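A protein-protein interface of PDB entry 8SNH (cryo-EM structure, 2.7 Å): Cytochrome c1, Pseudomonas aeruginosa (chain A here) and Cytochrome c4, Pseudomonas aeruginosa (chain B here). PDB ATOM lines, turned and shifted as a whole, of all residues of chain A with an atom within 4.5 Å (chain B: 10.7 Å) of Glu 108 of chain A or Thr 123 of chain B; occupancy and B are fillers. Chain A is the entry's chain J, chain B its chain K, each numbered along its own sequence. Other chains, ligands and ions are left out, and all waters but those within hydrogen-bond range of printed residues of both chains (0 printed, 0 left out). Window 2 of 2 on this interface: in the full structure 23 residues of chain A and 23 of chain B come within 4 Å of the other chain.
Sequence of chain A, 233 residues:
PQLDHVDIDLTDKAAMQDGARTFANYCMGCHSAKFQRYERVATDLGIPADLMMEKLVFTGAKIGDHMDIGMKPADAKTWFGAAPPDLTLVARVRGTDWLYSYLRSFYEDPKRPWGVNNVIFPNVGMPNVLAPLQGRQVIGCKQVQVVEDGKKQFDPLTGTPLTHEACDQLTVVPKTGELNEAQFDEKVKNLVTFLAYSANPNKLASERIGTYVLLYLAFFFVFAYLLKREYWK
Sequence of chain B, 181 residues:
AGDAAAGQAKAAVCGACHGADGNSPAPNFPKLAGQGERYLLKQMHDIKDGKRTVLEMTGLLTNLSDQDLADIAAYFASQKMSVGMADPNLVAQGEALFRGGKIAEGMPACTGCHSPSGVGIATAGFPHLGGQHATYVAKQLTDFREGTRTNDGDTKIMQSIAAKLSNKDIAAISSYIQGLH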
ATOM      1  N   TYR A 107     -22.975 -19.875 -17.946  1.00  0.00           N
ATOM      2  CA  TYR A 107     -21.741 -19.909 -18.719  1.00  0.00           C
ATOM      3  C   TYR A 107     -21.172 -18.502 -18.831  1.00  0.00           C
ATOM      4  O   TYR A 107     -21.911 -17.518 -18.871  1.00  0.00           O
ATOM      5  CB  TYR A 107     -21.963 -20.494 -20.118  1.00  0.00           C
ATOM      6  CG  TYR A 107     -22.935 -19.713 -20.973  1.00  0.00           C
ATOM      7  CD1 TYR A 107     -22.490 -18.713 -21.824  1.00  0.00           C
ATOM      8  CD2 TYR A 107     -24.296 -19.979 -20.930  1.00  0.00           C
ATOM      9  CE1 TYR A 107     -23.371 -17.998 -22.607  1.00  0.00           C
ATOM     10  CE2 TYR A 107     -25.185 -19.268 -21.709  1.00  0.00           C
ATOM     11  CZ  TYR A 107     -24.718 -18.280 -22.547  1.00  0.00           C
ATOM     12  OH  TYR A 107     -25.600 -17.569 -23.324  1.00  0.00           O
ATOM     13  N   GLU A 108     -19.847 -18.421 -18.910  1.00  0.00           N
ATOM     14  CA  GLU A 108     -19.181 -17.126 -18.942  1.00  0.00           C
ATOM     15  C   GLU A 108     -19.633 -16.317 -20.150  1.00  0.00           C
ATOM     16  O   GLU A 108     -19.711 -16.833 -21.269  1.00  0.00           O
ATOM     17  CB  GLU A 108     -17.665 -17.317 -18.964  1.00  0.00           C
ATOM     18  CG  GLU A 108     -17.125 -18.004 -17.722  1.00  0.00           C
ATOM     19  CD  GLU A 108     -15.620 -17.889 -17.596  1.00  0.00           C
ATOM     20  OE1 GLU A 108     -15.119 -16.757 -17.429  1.00  0.00           O
ATOM     21  OE2 GLU A 108     -14.938 -18.932 -17.659  1.00  0.00           O
ATOM     22  N   ASP A 109     -19.929 -15.040 -19.917  1.00  0.00           N
ATOM     23  CA  ASP A 109     -20.406 -14.143 -20.969  1.00  0.00           C
ATOM     24  C   ASP A 109     -19.926 -12.739 -20.642  1.00  0.00           C
ATOM     25  O   ASP A 109     -20.593 -11.991 -19.915  1.00  0.00           O
ATOM     26  CB  ASP A 109     -21.927 -14.183 -21.095  1.00  0.00           C
ATOM     27  CG  ASP A 109     -22.429 -13.470 -22.333  1.00  0.00           C
ATOM     28  OD1 ASP A 109     -21.594 -12.989 -23.127  1.00  0.00           O
ATOM     29  OD2 ASP A 109     -23.662 -13.389 -22.515  1.00  0.00           O
ATOM     30  N   PRO A 110     -18.763 -12.338 -21.166  1.00  0.00           N
ATOM     31  CA  PRO A 110     -18.202 -11.035 -20.773  1.00  0.00           C
ATOM     32  C   PRO A 110     -19.120  -9.862 -21.063  1.00  0.00           C
ATOM     33  O   PRO A 110     -19.019  -8.828 -20.391  1.00  0.00           O
ATOM     34  CB  PRO A 110     -16.905 -10.952 -21.589  1.00  0.00           C
ATOM     35  CG  PRO A 110     -16.559 -12.363 -21.909  1.00  0.00           C
ATOM     36  CD  PRO A 110     -17.862 -13.078 -22.065  1.00  0.00           C
ATOM     37  N   TRP A 114     -22.533  -9.366 -14.870  1.00  0.00           N
ATOM     38  CA  TRP A 114     -21.808 -10.234 -13.953  1.00  0.00           C
ATOM     39  C   TRP A 114     -20.941 -11.253 -14.675  1.00  0.00           C
ATOM     40  O   TRP A 114     -20.511 -12.233 -14.060  1.00  0.00           O
ATOM     41  CB  TRP A 114     -22.789 -10.941 -13.015  1.00  0.00           C
ATOM     42  CG  TRP A 114     -23.729  -9.993 -12.347  1.00  0.00           C
ATOM     43  CD1 TRP A 114     -25.087 -10.076 -12.307  1.00  0.00           C
ATOM     44  CD2 TRP A 114     -23.377  -8.805 -11.629  1.00  0.00           C
ATOM     45  NE1 TRP A 114     -25.604  -9.015 -11.606  1.00  0.00           N
ATOM     46  CE2 TRP A 114     -24.574  -8.220 -11.179  1.00  0.00           C
ATOM     47  CE3 TRP A 114     -22.165  -8.181 -11.322  1.00  0.00           C
ATOM     48  CZ2 TRP A 114     -24.594  -7.043 -10.438  1.00  0.00           C
ATOM     49  CZ3 TRP A 114     -22.188  -7.014 -10.588  1.00  0.00           C
ATOM     50  CH2 TRP A 114     -23.394  -6.457 -10.153  1.00  0.00           C
ATOM     51  N   GLY A 115     -20.678 -11.046 -15.963  1.00  0.00           N
ATOM     52  CA  GLY A 115     -19.764 -11.899 -16.690  1.00  0.00           C
ATOM     53  C   GLY A 115     -20.306 -13.262 -17.046  1.00  0.00           C
ATOM     54  O   GLY A 115     -19.551 -14.096 -17.551  1.00  0.00           O
ATOM     55  N   VAL A 116     -21.591 -13.519 -16.798  1.00  0.00           N
ATOM     56  CA  VAL A 116     -22.191 -14.814 -17.081  1.00  0.00           C
ATOM     57  C   VAL A 116     -23.575 -14.606 -17.679  1.00  0.00           C
ATOM     58  O   VAL A 116     -24.216 -13.572 -17.489  1.00  0.00           O
ATOM     59  CB  VAL A 116     -22.294 -15.705 -15.822  1.00  0.00           C
ATOM     60  CG1 VAL A 116     -20.908 -16.064 -15.309  1.00  0.00           C
ATOM     61  CG2 VAL A 116     -23.115 -15.016 -14.743  1.00  0.00           C
ATOM     62  N   ARG A 136     -15.461 -23.191 -14.224  1.00  0.00           N
ATOM     63  CA  ARG A 136     -15.734 -22.299 -15.343  1.00  0.00           C
ATOM     64  C   ARG A 136     -16.466 -23.054 -16.446  1.00  0.00           C
ATOM     65  O   ARG A 136     -15.950 -24.042 -16.978  1.00  0.00           O
ATOM     66  CB  ARG A 136     -14.432 -21.704 -15.870  1.00  0.00           C
ATOM     67  CG  ARG A 136     -13.680 -20.864 -14.847  1.00  0.00           C
ATOM     68  CD  ARG A 136     -12.445 -20.205 -15.446  1.00  0.00           C
ATOM     69  NE  ARG A 136     -12.739 -19.505 -16.693  1.00  0.00           N
ATOM     70  CZ  ARG A 136     -12.213 -19.794 -17.877  1.00  0.00           C
ATOM     71  NH1 ARG A 136     -11.335 -20.773 -18.030  1.00  0.00           N
ATOM     72  NH2 ARG A 136     -12.576 -19.079 -18.937  1.00  0.00           N
ATOM     73  N   GLN A 137     -17.662 -22.589 -16.789  1.00  0.00           N
ATOM     74  CA  GLN A 137     -18.465 -23.164 -17.860  1.00  0.00           C
ATOM     75  C   GLN A 137     -18.572 -22.154 -18.994  1.00  0.00           C
ATOM     76  O   GLN A 137     -18.815 -20.968 -18.752  1.00  0.00           O
ATOM     77  CB  GLN A 137     -19.855 -23.556 -17.353  1.00  0.00           C
ATOM     78  CG  GLN A 137     -20.713 -24.264 -18.386  1.00  0.00           C
ATOM     79  CD  GLN A 137     -21.887 -24.999 -17.770  1.00  0.00           C
ATOM     80  OE1 GLN A 137     -21.921 -26.228 -17.748  1.00  0.00           O
ATOM     81  NE2 GLN A 137     -22.860 -24.248 -17.269  1.00  0.00           N
ATOM     82  N   VAL A 138     -18.379 -22.625 -20.228  1.00  0.00           N
ATOM     83  CA  VAL A 138     -18.301 -21.761 -21.397  1.00  0.00           C
ATOM     84  C   VAL A 138     -19.094 -22.375 -22.543  1.00  0.00           C
ATOM     85  O   VAL A 138     -19.390 -23.571 -22.559  1.00  0.00           O
ATOM     86  CB  VAL A 138     -16.841 -21.518 -21.837  1.00  0.00           C
ATOM     87  CG1 VAL A 138     -16.102 -20.701 -20.792  1.00  0.00           C
ATOM     88  CG2 VAL A 138     -16.135 -22.843 -22.090  1.00  0.00           C
ATOM     89  N   ALA B   1      -8.024 -11.015 -22.653  1.00  0.00           N
ATOM     90  CA  ALA B   1      -7.542 -11.597 -21.406  1.00  0.00           C
ATOM     91  C   ALA B   1      -6.032 -11.425 -21.283  1.00  0.00           C
ATOM     92  O   ALA B   1      -5.311 -11.460 -22.280  1.00  0.00           O
ATOM     93  CB  ALA B   1      -7.917 -13.068 -21.329  1.00  0.00           C
ATOM     94  N   GLY B  34      -4.608 -14.796  -5.999  1.00  0.00           N
ATOM     95  CA  GLY B  34      -5.897 -15.449  -6.034  1.00  0.00           C
ATOM     96  C   GLY B  34      -7.082 -14.522  -6.170  1.00  0.00           C
ATOM     97  O   GLY B  34      -8.218 -15.005  -6.200  1.00  0.00           O
ATOM     98  N   GLN B  35      -6.861 -13.215  -6.252  1.00  0.00           N
ATOM     99  CA  GLN B  35      -7.963 -12.284  -6.428  1.00  0.00           C
ATOM    100  C   GLN B  35      -8.503 -12.372  -7.849  1.00  0.00           C
ATOM    101  O   GLN B  35      -7.767 -12.640  -8.802  1.00  0.00           O
ATOM    102  CB  GLN B  35      -7.509 -10.857  -6.121  1.00  0.00           C
ATOM    103  CG  GLN B  35      -8.626  -9.825  -6.122  1.00  0.00           C
ATOM    104  CD  GLN B  35      -9.770 -10.202  -5.209  1.00  0.00           C
ATOM    105  OE1 GLN B  35     -10.703 -10.889  -5.619  1.00  0.00           O
ATOM    106  NE2 GLN B  35      -9.706  -9.755  -3.963  1.00  0.00           N
ATOM    107  N   GLY B  36      -9.806 -12.149  -7.985  1.00  0.00           N
ATOM    108  CA  GLY B  36     -10.444 -12.222  -9.284  1.00  0.00           C
ATOM    109  C   GLY B  36      -9.780 -11.313 -10.295  1.00  0.00           C
ATOM    110  O   GLY B  36      -9.505 -10.146 -10.003  1.00  0.00           O
ATOM    111  N   GLU B  37      -9.515 -11.839 -11.493  1.00  0.00           N
ATOM    112  CA  GLU B  37      -8.836 -11.041 -12.508  1.00  0.00           C
ATOM    113  C   GLU B  37      -9.666  -9.825 -12.892  1.00  0.00           C
ATOM    114  O   GLU B  37      -9.128  -8.724 -13.059  1.00  0.00           O
ATOM    115  CB  GLU B  37      -8.535 -11.899 -13.736  1.00  0.00           C
ATOM    116  CG  GLU B  37      -8.266 -11.099 -15.000  1.00  0.00           C
ATOM    117  CD  GLU B  37      -7.443 -11.866 -16.016  1.00  0.00           C
ATOM    118  OE1 GLU B  37      -7.320 -13.101 -15.876  1.00  0.00           O
ATOM    119  OE2 GLU B  37      -6.917 -11.233 -16.956  1.00  0.00           O
ATOM    120  N   ARG B  38     -10.981  -9.998 -13.032  1.00  0.00           N
ATOM    121  CA  ARG B  38     -11.842  -8.863 -13.343  1.00  0.00           C
ATOM    122  C   ARG B  38     -11.759  -7.804 -12.252  1.00  0.00           C
ATOM    123  O   ARG B  38     -11.617  -6.610 -12.538  1.00  0.00           O
ATOM    124  CB  ARG B  38     -13.286  -9.334 -13.525  1.00  0.00           C
ATOM    125  CG  ARG B  38     -14.303  -8.204 -13.546  1.00  0.00           C
ATOM    126  CD  ARG B  38     -15.678  -8.687 -13.964  1.00  0.00           C
ATOM    127  NE  ARG B  38     -16.666  -7.617 -13.919  1.00  0.00           N
ATOM    128  CZ  ARG B  38     -17.959  -7.777 -14.171  1.00  0.00           C
ATOM    129  NH1 ARG B  38     -18.459  -8.958 -14.496  1.00  0.00           N
ATOM    130  NH2 ARG B  38     -18.769  -6.727 -14.093  1.00  0.00           N
ATOM    131  N   TYR B  39     -11.846  -8.224 -10.987  1.00  0.00           N
ATOM    132  CA  TYR B  39     -11.783  -7.265  -9.891  1.00  0.00           C
ATOM    133  C   TYR B  39     -10.422  -6.584  -9.829  1.00  0.00           C
ATOM    134  O   TYR B  39     -10.338  -5.372  -9.610  1.00  0.00           O
ATOM    135  CB  TYR B  39     -12.085  -7.954  -8.562  1.00  0.00           C
ATOM    136  CG  TYR B  39     -11.898  -7.039  -7.375  1.00  0.00           C
ATOM    137  CD1 TYR B  39     -12.895  -6.153  -6.997  1.00  0.00           C
ATOM    138  CD2 TYR B  39     -10.716  -7.043  -6.648  1.00  0.00           C
ATOM    139  CE1 TYR B  39     -12.727  -5.309  -5.923  1.00  0.00           C
ATOM    140  CE2 TYR B  39     -10.539  -6.199  -5.570  1.00  0.00           C
ATOM    141  CZ  TYR B  39     -11.549  -5.334  -5.215  1.00  0.00           C
ATOM    142  OH  TYR B  39     -11.389  -4.489  -4.145  1.00  0.00           O
ATOM    143  N   LEU B  40      -9.343  -7.352  -9.999  1.00  0.00           N
ATOM    144  CA  LEU B  40      -8.009  -6.762  -9.972  1.00  0.00           C
ATOM    145  C   LEU B  40      -7.856  -5.720 -11.071  1.00  0.00           C
ATOM    146  O   LEU B  40      -7.333  -4.622 -10.839  1.00  0.00           O
ATOM    147  CB  LEU B  40      -6.952  -7.855 -10.125  1.00  0.00           C
ATOM    148  CG  LEU B  40      -6.587  -8.664  -8.882  1.00  0.00           C
ATOM    149  CD1 LEU B  40      -5.694  -9.832  -9.266  1.00  0.00           C
ATOM    150  CD2 LEU B  40      -5.907  -7.793  -7.841  1.00  0.00           C
ATOM    151  N   LEU B  41      -8.307  -6.053 -12.281  1.00  0.00           N
ATOM    152  CA  LEU B  41      -8.203  -5.116 -13.391  1.00  0.00           C
ATOM    153  C   LEU B  41      -9.042  -3.872 -13.134  1.00  0.00           C
ATOM    154  O   LEU B  41      -8.607  -2.751 -13.420  1.00  0.00           O
ATOM    155  CB  LEU B  41      -8.630  -5.802 -14.689  1.00  0.00           C
ATOM    156  CG  LEU B  41      -8.208  -5.143 -16.004  1.00  0.00           C
ATOM    157  CD1 LEU B  41      -6.698  -4.965 -16.065  1.00  0.00           C
ATOM    158  CD2 LEU B  41      -8.697  -5.964 -17.184  1.00  0.00           C
ATOM    159  N   LYS B  42     -10.248  -4.048 -12.589  1.00  0.00           N
ATOM    160  CA  LYS B  42     -11.083  -2.895 -12.273  1.00  0.00           C
ATOM    161  C   LYS B  42     -10.411  -1.998 -11.243  1.00  0.00           C
ATOM    162  O   LYS B  42     -10.422  -0.772 -11.380  1.00  0.00           O
ATOM    163  CB  LYS B  42     -12.450  -3.353 -11.765  1.00  0.00           C
ATOM    164  CG  LYS B  42     -13.374  -2.212 -11.365  1.00  0.00           C
ATOM    165  CD  LYS B  42     -14.606  -2.713 -10.640  1.00  0.00           C
ATOM    166  CE  LYS B  42     -15.604  -1.590 -10.416  1.00  0.00           C
ATOM    167  NZ  LYS B  42     -15.019  -0.471  -9.631  1.00  0.00           N
ATOM    168  N   ALA B  77      -4.223 -13.299 -10.341  1.00  0.00           N
ATOM    169  CA  ALA B  77      -5.375 -14.186 -10.257  1.00  0.00           C
ATOM    170  C   ALA B  77      -4.986 -15.651 -10.390  1.00  0.00           C
ATOM    171  O   ALA B  77      -5.759 -16.523  -9.981  1.00  0.00           O
ATOM    172  CB  ALA B  77      -6.395 -13.827 -11.338  1.00  0.00           C
ATOM    173  N   GLY B 112     -23.348 -14.163   0.017  1.00  0.00           N
ATOM    174  CA  GLY B 112     -23.998 -14.141  -1.277  1.00  0.00           C
ATOM    175  C   GLY B 112     -23.076 -13.678  -2.385  1.00  0.00           C
ATOM    176  O   GLY B 112     -22.735 -14.450  -3.285  1.00  0.00           O
ATOM    177  N   CYS B 113     -22.665 -12.412  -2.327  1.00  0.00           N
ATOM    178  CA  CYS B 113     -21.797 -11.869  -3.366  1.00  0.00           C
ATOM    179  C   CYS B 113     -20.376 -12.398  -3.227  1.00  0.00           C
ATOM    180  O   CYS B 113     -19.743 -12.764  -4.222  1.00  0.00           O
ATOM    181  CB  CYS B 113     -21.813 -10.348  -3.300  1.00  0.00           C
ATOM    182  SG  CYS B 113     -23.471  -9.644  -3.113  1.00  0.00           S
ATOM    183  N   SER B 115     -18.359 -15.563  -1.755  1.00  0.00           N
ATOM    184  CA  SER B 115     -18.807 -16.922  -1.510  1.00  0.00           C
ATOM    185  C   SER B 115     -18.875 -17.209  -0.011  1.00  0.00           C
ATOM    186  O   SER B 115     -18.330 -16.460   0.803  1.00  0.00           O
ATOM    187  CB  SER B 115     -17.867 -17.915  -2.185  1.00  0.00           C
ATOM    188  OG  SER B 115     -17.997 -17.856  -3.592  1.00  0.00           O
ATOM    189  N   VAL B 119     -14.337 -16.734  -1.449  1.00  0.00           N
ATOM    190  CA  VAL B 119     -13.576 -16.675  -2.695  1.00  0.00           C
ATOM    191  C   VAL B 119     -14.117 -15.646  -3.672  1.00  0.00           C
ATOM    192  O   VAL B 119     -13.498 -15.421  -4.718  1.00  0.00           O
ATOM    193  CB  VAL B 119     -13.545 -18.043  -3.404  1.00  0.00           C
ATOM    194  CG1 VAL B 119     -12.752 -19.046  -2.585  1.00  0.00           C
ATOM    195  CG2 VAL B 119     -14.955 -18.558  -3.660  1.00  0.00           C
ATOM    196  N   GLY B 120     -15.246 -15.018  -3.370  1.00  0.00           N
ATOM    197  CA  GLY B 120     -15.825 -14.076  -4.299  1.00  0.00           C
ATOM    198  C   GLY B 120     -16.377 -14.776  -5.530  1.00  0.00           C
ATOM    199  O   GLY B 120     -16.452 -16.001  -5.616  1.00  0.00           O
ATOM    200  N   ILE B 121     -16.774 -13.956  -6.494  1.00  0.00           N
ATOM    201  CA  ILE B 121     -17.234 -14.422  -7.798  1.00  0.00           C
ATOM    202  C   ILE B 121     -16.358 -13.724  -8.829  1.00  0.00           C
ATOM    203  O   ILE B 121     -16.523 -12.528  -9.095  1.00  0.00           O
ATOM    204  CB  ILE B 121     -18.721 -14.138  -8.032  1.00  0.00           C
ATOM    205  CG1 ILE B 121     -19.540 -14.601  -6.825  1.00  0.00           C
ATOM    206  CG2 ILE B 121     -19.202 -14.839  -9.292  1.00  0.00           C
ATOM    207  CD1 ILE B 121     -21.033 -14.436  -6.990  1.00  0.00           C
ATOM    208  N   ALA B 122     -15.418 -14.470  -9.413  1.00  0.00           N
ATOM    209  CA  ALA B 122     -14.438 -13.861 -10.303  1.00  0.00           C
ATOM    210  C   ALA B 122     -15.103 -13.233 -11.520  1.00  0.00           C
ATOM    211  O   ALA B 122     -14.762 -12.112 -11.913  1.00  0.00           O
ATOM    212  CB  ALA B 122     -13.409 -14.905 -10.733  1.00  0.00           C
ATOM    213  N   THR B 123     -16.056 -13.938 -12.132  1.00  0.00           N
ATOM    214  CA  THR B 123     -16.706 -13.410 -13.327  1.00  0.00           C
ATOM    215  C   THR B 123     -17.504 -12.152 -13.014  1.00  0.00           C
ATOM    216  O   THR B 123     -17.497 -11.194 -13.794  1.00  0.00           O
ATOM    217  CB  THR B 123     -17.611 -14.474 -13.948  1.00  0.00           C
ATOM    218  OG1 THR B 123     -18.451 -15.044 -12.937  1.00  0.00           O
ATOM    219  CG2 THR B 123     -16.780 -15.570 -14.592  1.00  0.00           C
ATOM    220  N   ALA B 124     -18.202 -12.135 -11.879  1.00  0.00           N
ATOM    221  CA  ALA B 124     -19.021 -10.990 -11.506  1.00  0.00           C
ATOM    222  C   ALA B 124     -18.204  -9.818 -10.984  1.00  0.00           C
ATOM    223  O   ALA B 124     -18.754  -8.723 -10.829  1.00  0.00           O
ATOM    224  CB  ALA B 124     -20.046 -11.398 -10.447  1.00  0.00           C
ATOM    225  N   GLY B 125     -16.917 -10.015 -10.715  1.00  0.00           N
ATOM    226  CA  GLY B 125     -16.103  -8.967 -10.143  1.00  0.00           C
ATOM    227  C   GLY B 125     -16.213  -8.829  -8.644  1.00  0.00           C
ATOM    228  O   GLY B 125     -15.651  -7.882  -8.086  1.00  0.00           O
ATOM    229  N   PHE B 126     -16.916  -9.733  -7.977  1.00  0.00           N
ATOM    230  CA  PHE B 126     -16.987  -9.697  -6.522  1.00  0.00           C
ATOM    231  C   PHE B 126     -15.660 -10.184  -5.954  1.00  0.00           C
ATOM    232  O   PHE B 126     -15.272 -11.330  -6.211  1.00  0.00           O
ATOM    233  CB  PHE B 126     -18.144 -10.559  -6.024  1.00  0.00           C
ATOM    234  CG  PHE B 126     -19.499 -10.105  -6.505  1.00  0.00           C
ATOM    235  CD1 PHE B 126     -19.710  -8.800  -6.921  1.00  0.00           C
ATOM    236  CD2 PHE B 126     -20.562 -10.990  -6.541  1.00  0.00           C
ATOM    237  CE1 PHE B 126     -20.953  -8.391  -7.359  1.00  0.00           C
ATOM    238  CE2 PHE B 126     -21.808 -10.583  -6.977  1.00  0.00           C
ATOM    239  CZ  PHE B 126     -22.003  -9.283  -7.387  1.00  0.00           C
ATOM    240  N   PRO B 127     -14.936  -9.367  -5.194  1.00  0.00           N
ATOM    241  CA  PRO B 127     -13.561  -9.729  -4.836  1.00  0.00           C
ATOM    242  C   PRO B 127     -13.483 -10.927  -3.905  1.00  0.00           C
ATOM    243  O   PRO B 127     -14.348 -11.151  -3.057  1.00  0.00           O
ATOM    244  CB  PRO B 127     -13.030  -8.467  -4.147  1.00  0.00           C
ATOM    245  CG  PRO B 127     -14.229  -7.744  -3.686  1.00  0.00           C
ATOM    246  CD  PRO B 127     -15.314  -8.047  -4.663  1.00  0.00           C
ATOM    247  N   HIS B 128     -12.417 -11.701  -4.085  1.00  0.00           N
ATOM    248  CA  HIS B 128     -12.013 -12.676  -3.084  1.00  0.00           C
ATOM    249  C   HIS B 128     -11.734 -11.965  -1.767  1.00  0.00           C
ATOM    250  O   HIS B 128     -11.039 -10.945  -1.736  1.00  0.00           O
ATOM    251  CB  HIS B 128     -10.771 -13.426  -3.574  1.00  0.00           C
ATOM    252  CG  HIS B 128     -10.284 -14.488  -2.637  1.00  0.00           C
ATOM    253  ND1 HIS B 128     -10.128 -15.802  -3.025  1.00  0.00           N
ATOM    254  CD2 HIS B 128      -9.886 -14.429  -1.345  1.00  0.00           C
ATOM    255  CE1 HIS B 128      -9.675 -16.508  -2.006  1.00  0.00           C
ATOM    256  NE2 HIS B 128      -9.519 -15.698  -0.974  1.00  0.00           N
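O of Trp 114 of chain A is in hydrogen-bond range of N of Ala 124 of chain B, at 3.2 Å. The backbone carbonyl oxygen (O) of Trp 114 of chain A lies close to the backbone carbonyl oxygen (O) of Thr 123 of chain B (3.2 Å). NH1 of Arg 38 of chain B sits close to N of Gly 115 of chain A, 3.4 Å away.
NE of Arg 136 of chain A is in salt-bridge range of OE2 of Glu 108 of chain A, 2.5 Å away. The backbone carbonyl oxygen of Gln 137 of chain A sits at hydrogen-bond distance from the backbone NH of Glu 108 of chain A, at 2.8 Å. N of Asp 109 of chain A sits at hydrogen-bond distance from O of Gly 115 of chain A (2.6 Å). O of Thr 123 of chain B is in hydrogen-bond range of NH1 of Arg 38 of chain B, 2.5 Å away. The backbone carbonyl oxygen (O) of Ile 121 of chain B sits at hydrogen-bond distance from the backbone NH (N) of Phe 126 of chain B (3.0 Å).
Among the printed residues, merely in contact across the chains: Trp 114 of chain A with Arg 38 of chain B, Glu 108 of chain A with Thr 123 of chain B, Val 116 of chain A with Thr 123 of chain B, Trp 114 of chain A with Phe 126 of chain B and Gly 115 of chain A with Thr 123 of chain B.
Of chain A, only Glu 108 (3.5 Å), Trp 114 (3.2 Å), Gly 115 (3.7 Å) and Val 116 (3.6 Å) come within 4 Å of Thr 123 of chain B. No residue of chain B comes within 4 Å of Tyr 107 of chain A. No residue of chain B comes within 4 Å of Asp 109 of chain A. Val 116 of chain A touches one residue of chain B. Arg 136 of chain A touches none of the printed residues of chain B. Of the printed residues of chain A, Arg 38 of chain B touches Trp 114 and Gly 115. Printed residues of chain A within 4 Å of Phe 126 of chain B: Trp 114 (3.7 Å). Of the printed residues of chain A, Ala 124 of chain B touches Trp 114 (3.2 Å). Of the printed residues of chain B, Trp 114 of chain A touches Arg 38, Thr 123, Ala 124 and Phe 126. Pro 127 of chain B touches none of the printed residues of chain A.
Of the 10 printed residues of chain A, 4 touch a printed residue of chain B. Printed residues of chain A that touch a printed residue of chain B: Glu 108, Trp 114, Gly 115 and Val 116. Hydrophobic or aromatic side chains of chain A that line the printed part of chain B: Trp 114 and Val 116. Hydrophobic or aromatic side chains of chain B that line the printed part of chain A: Ala 124 and Phe 126.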
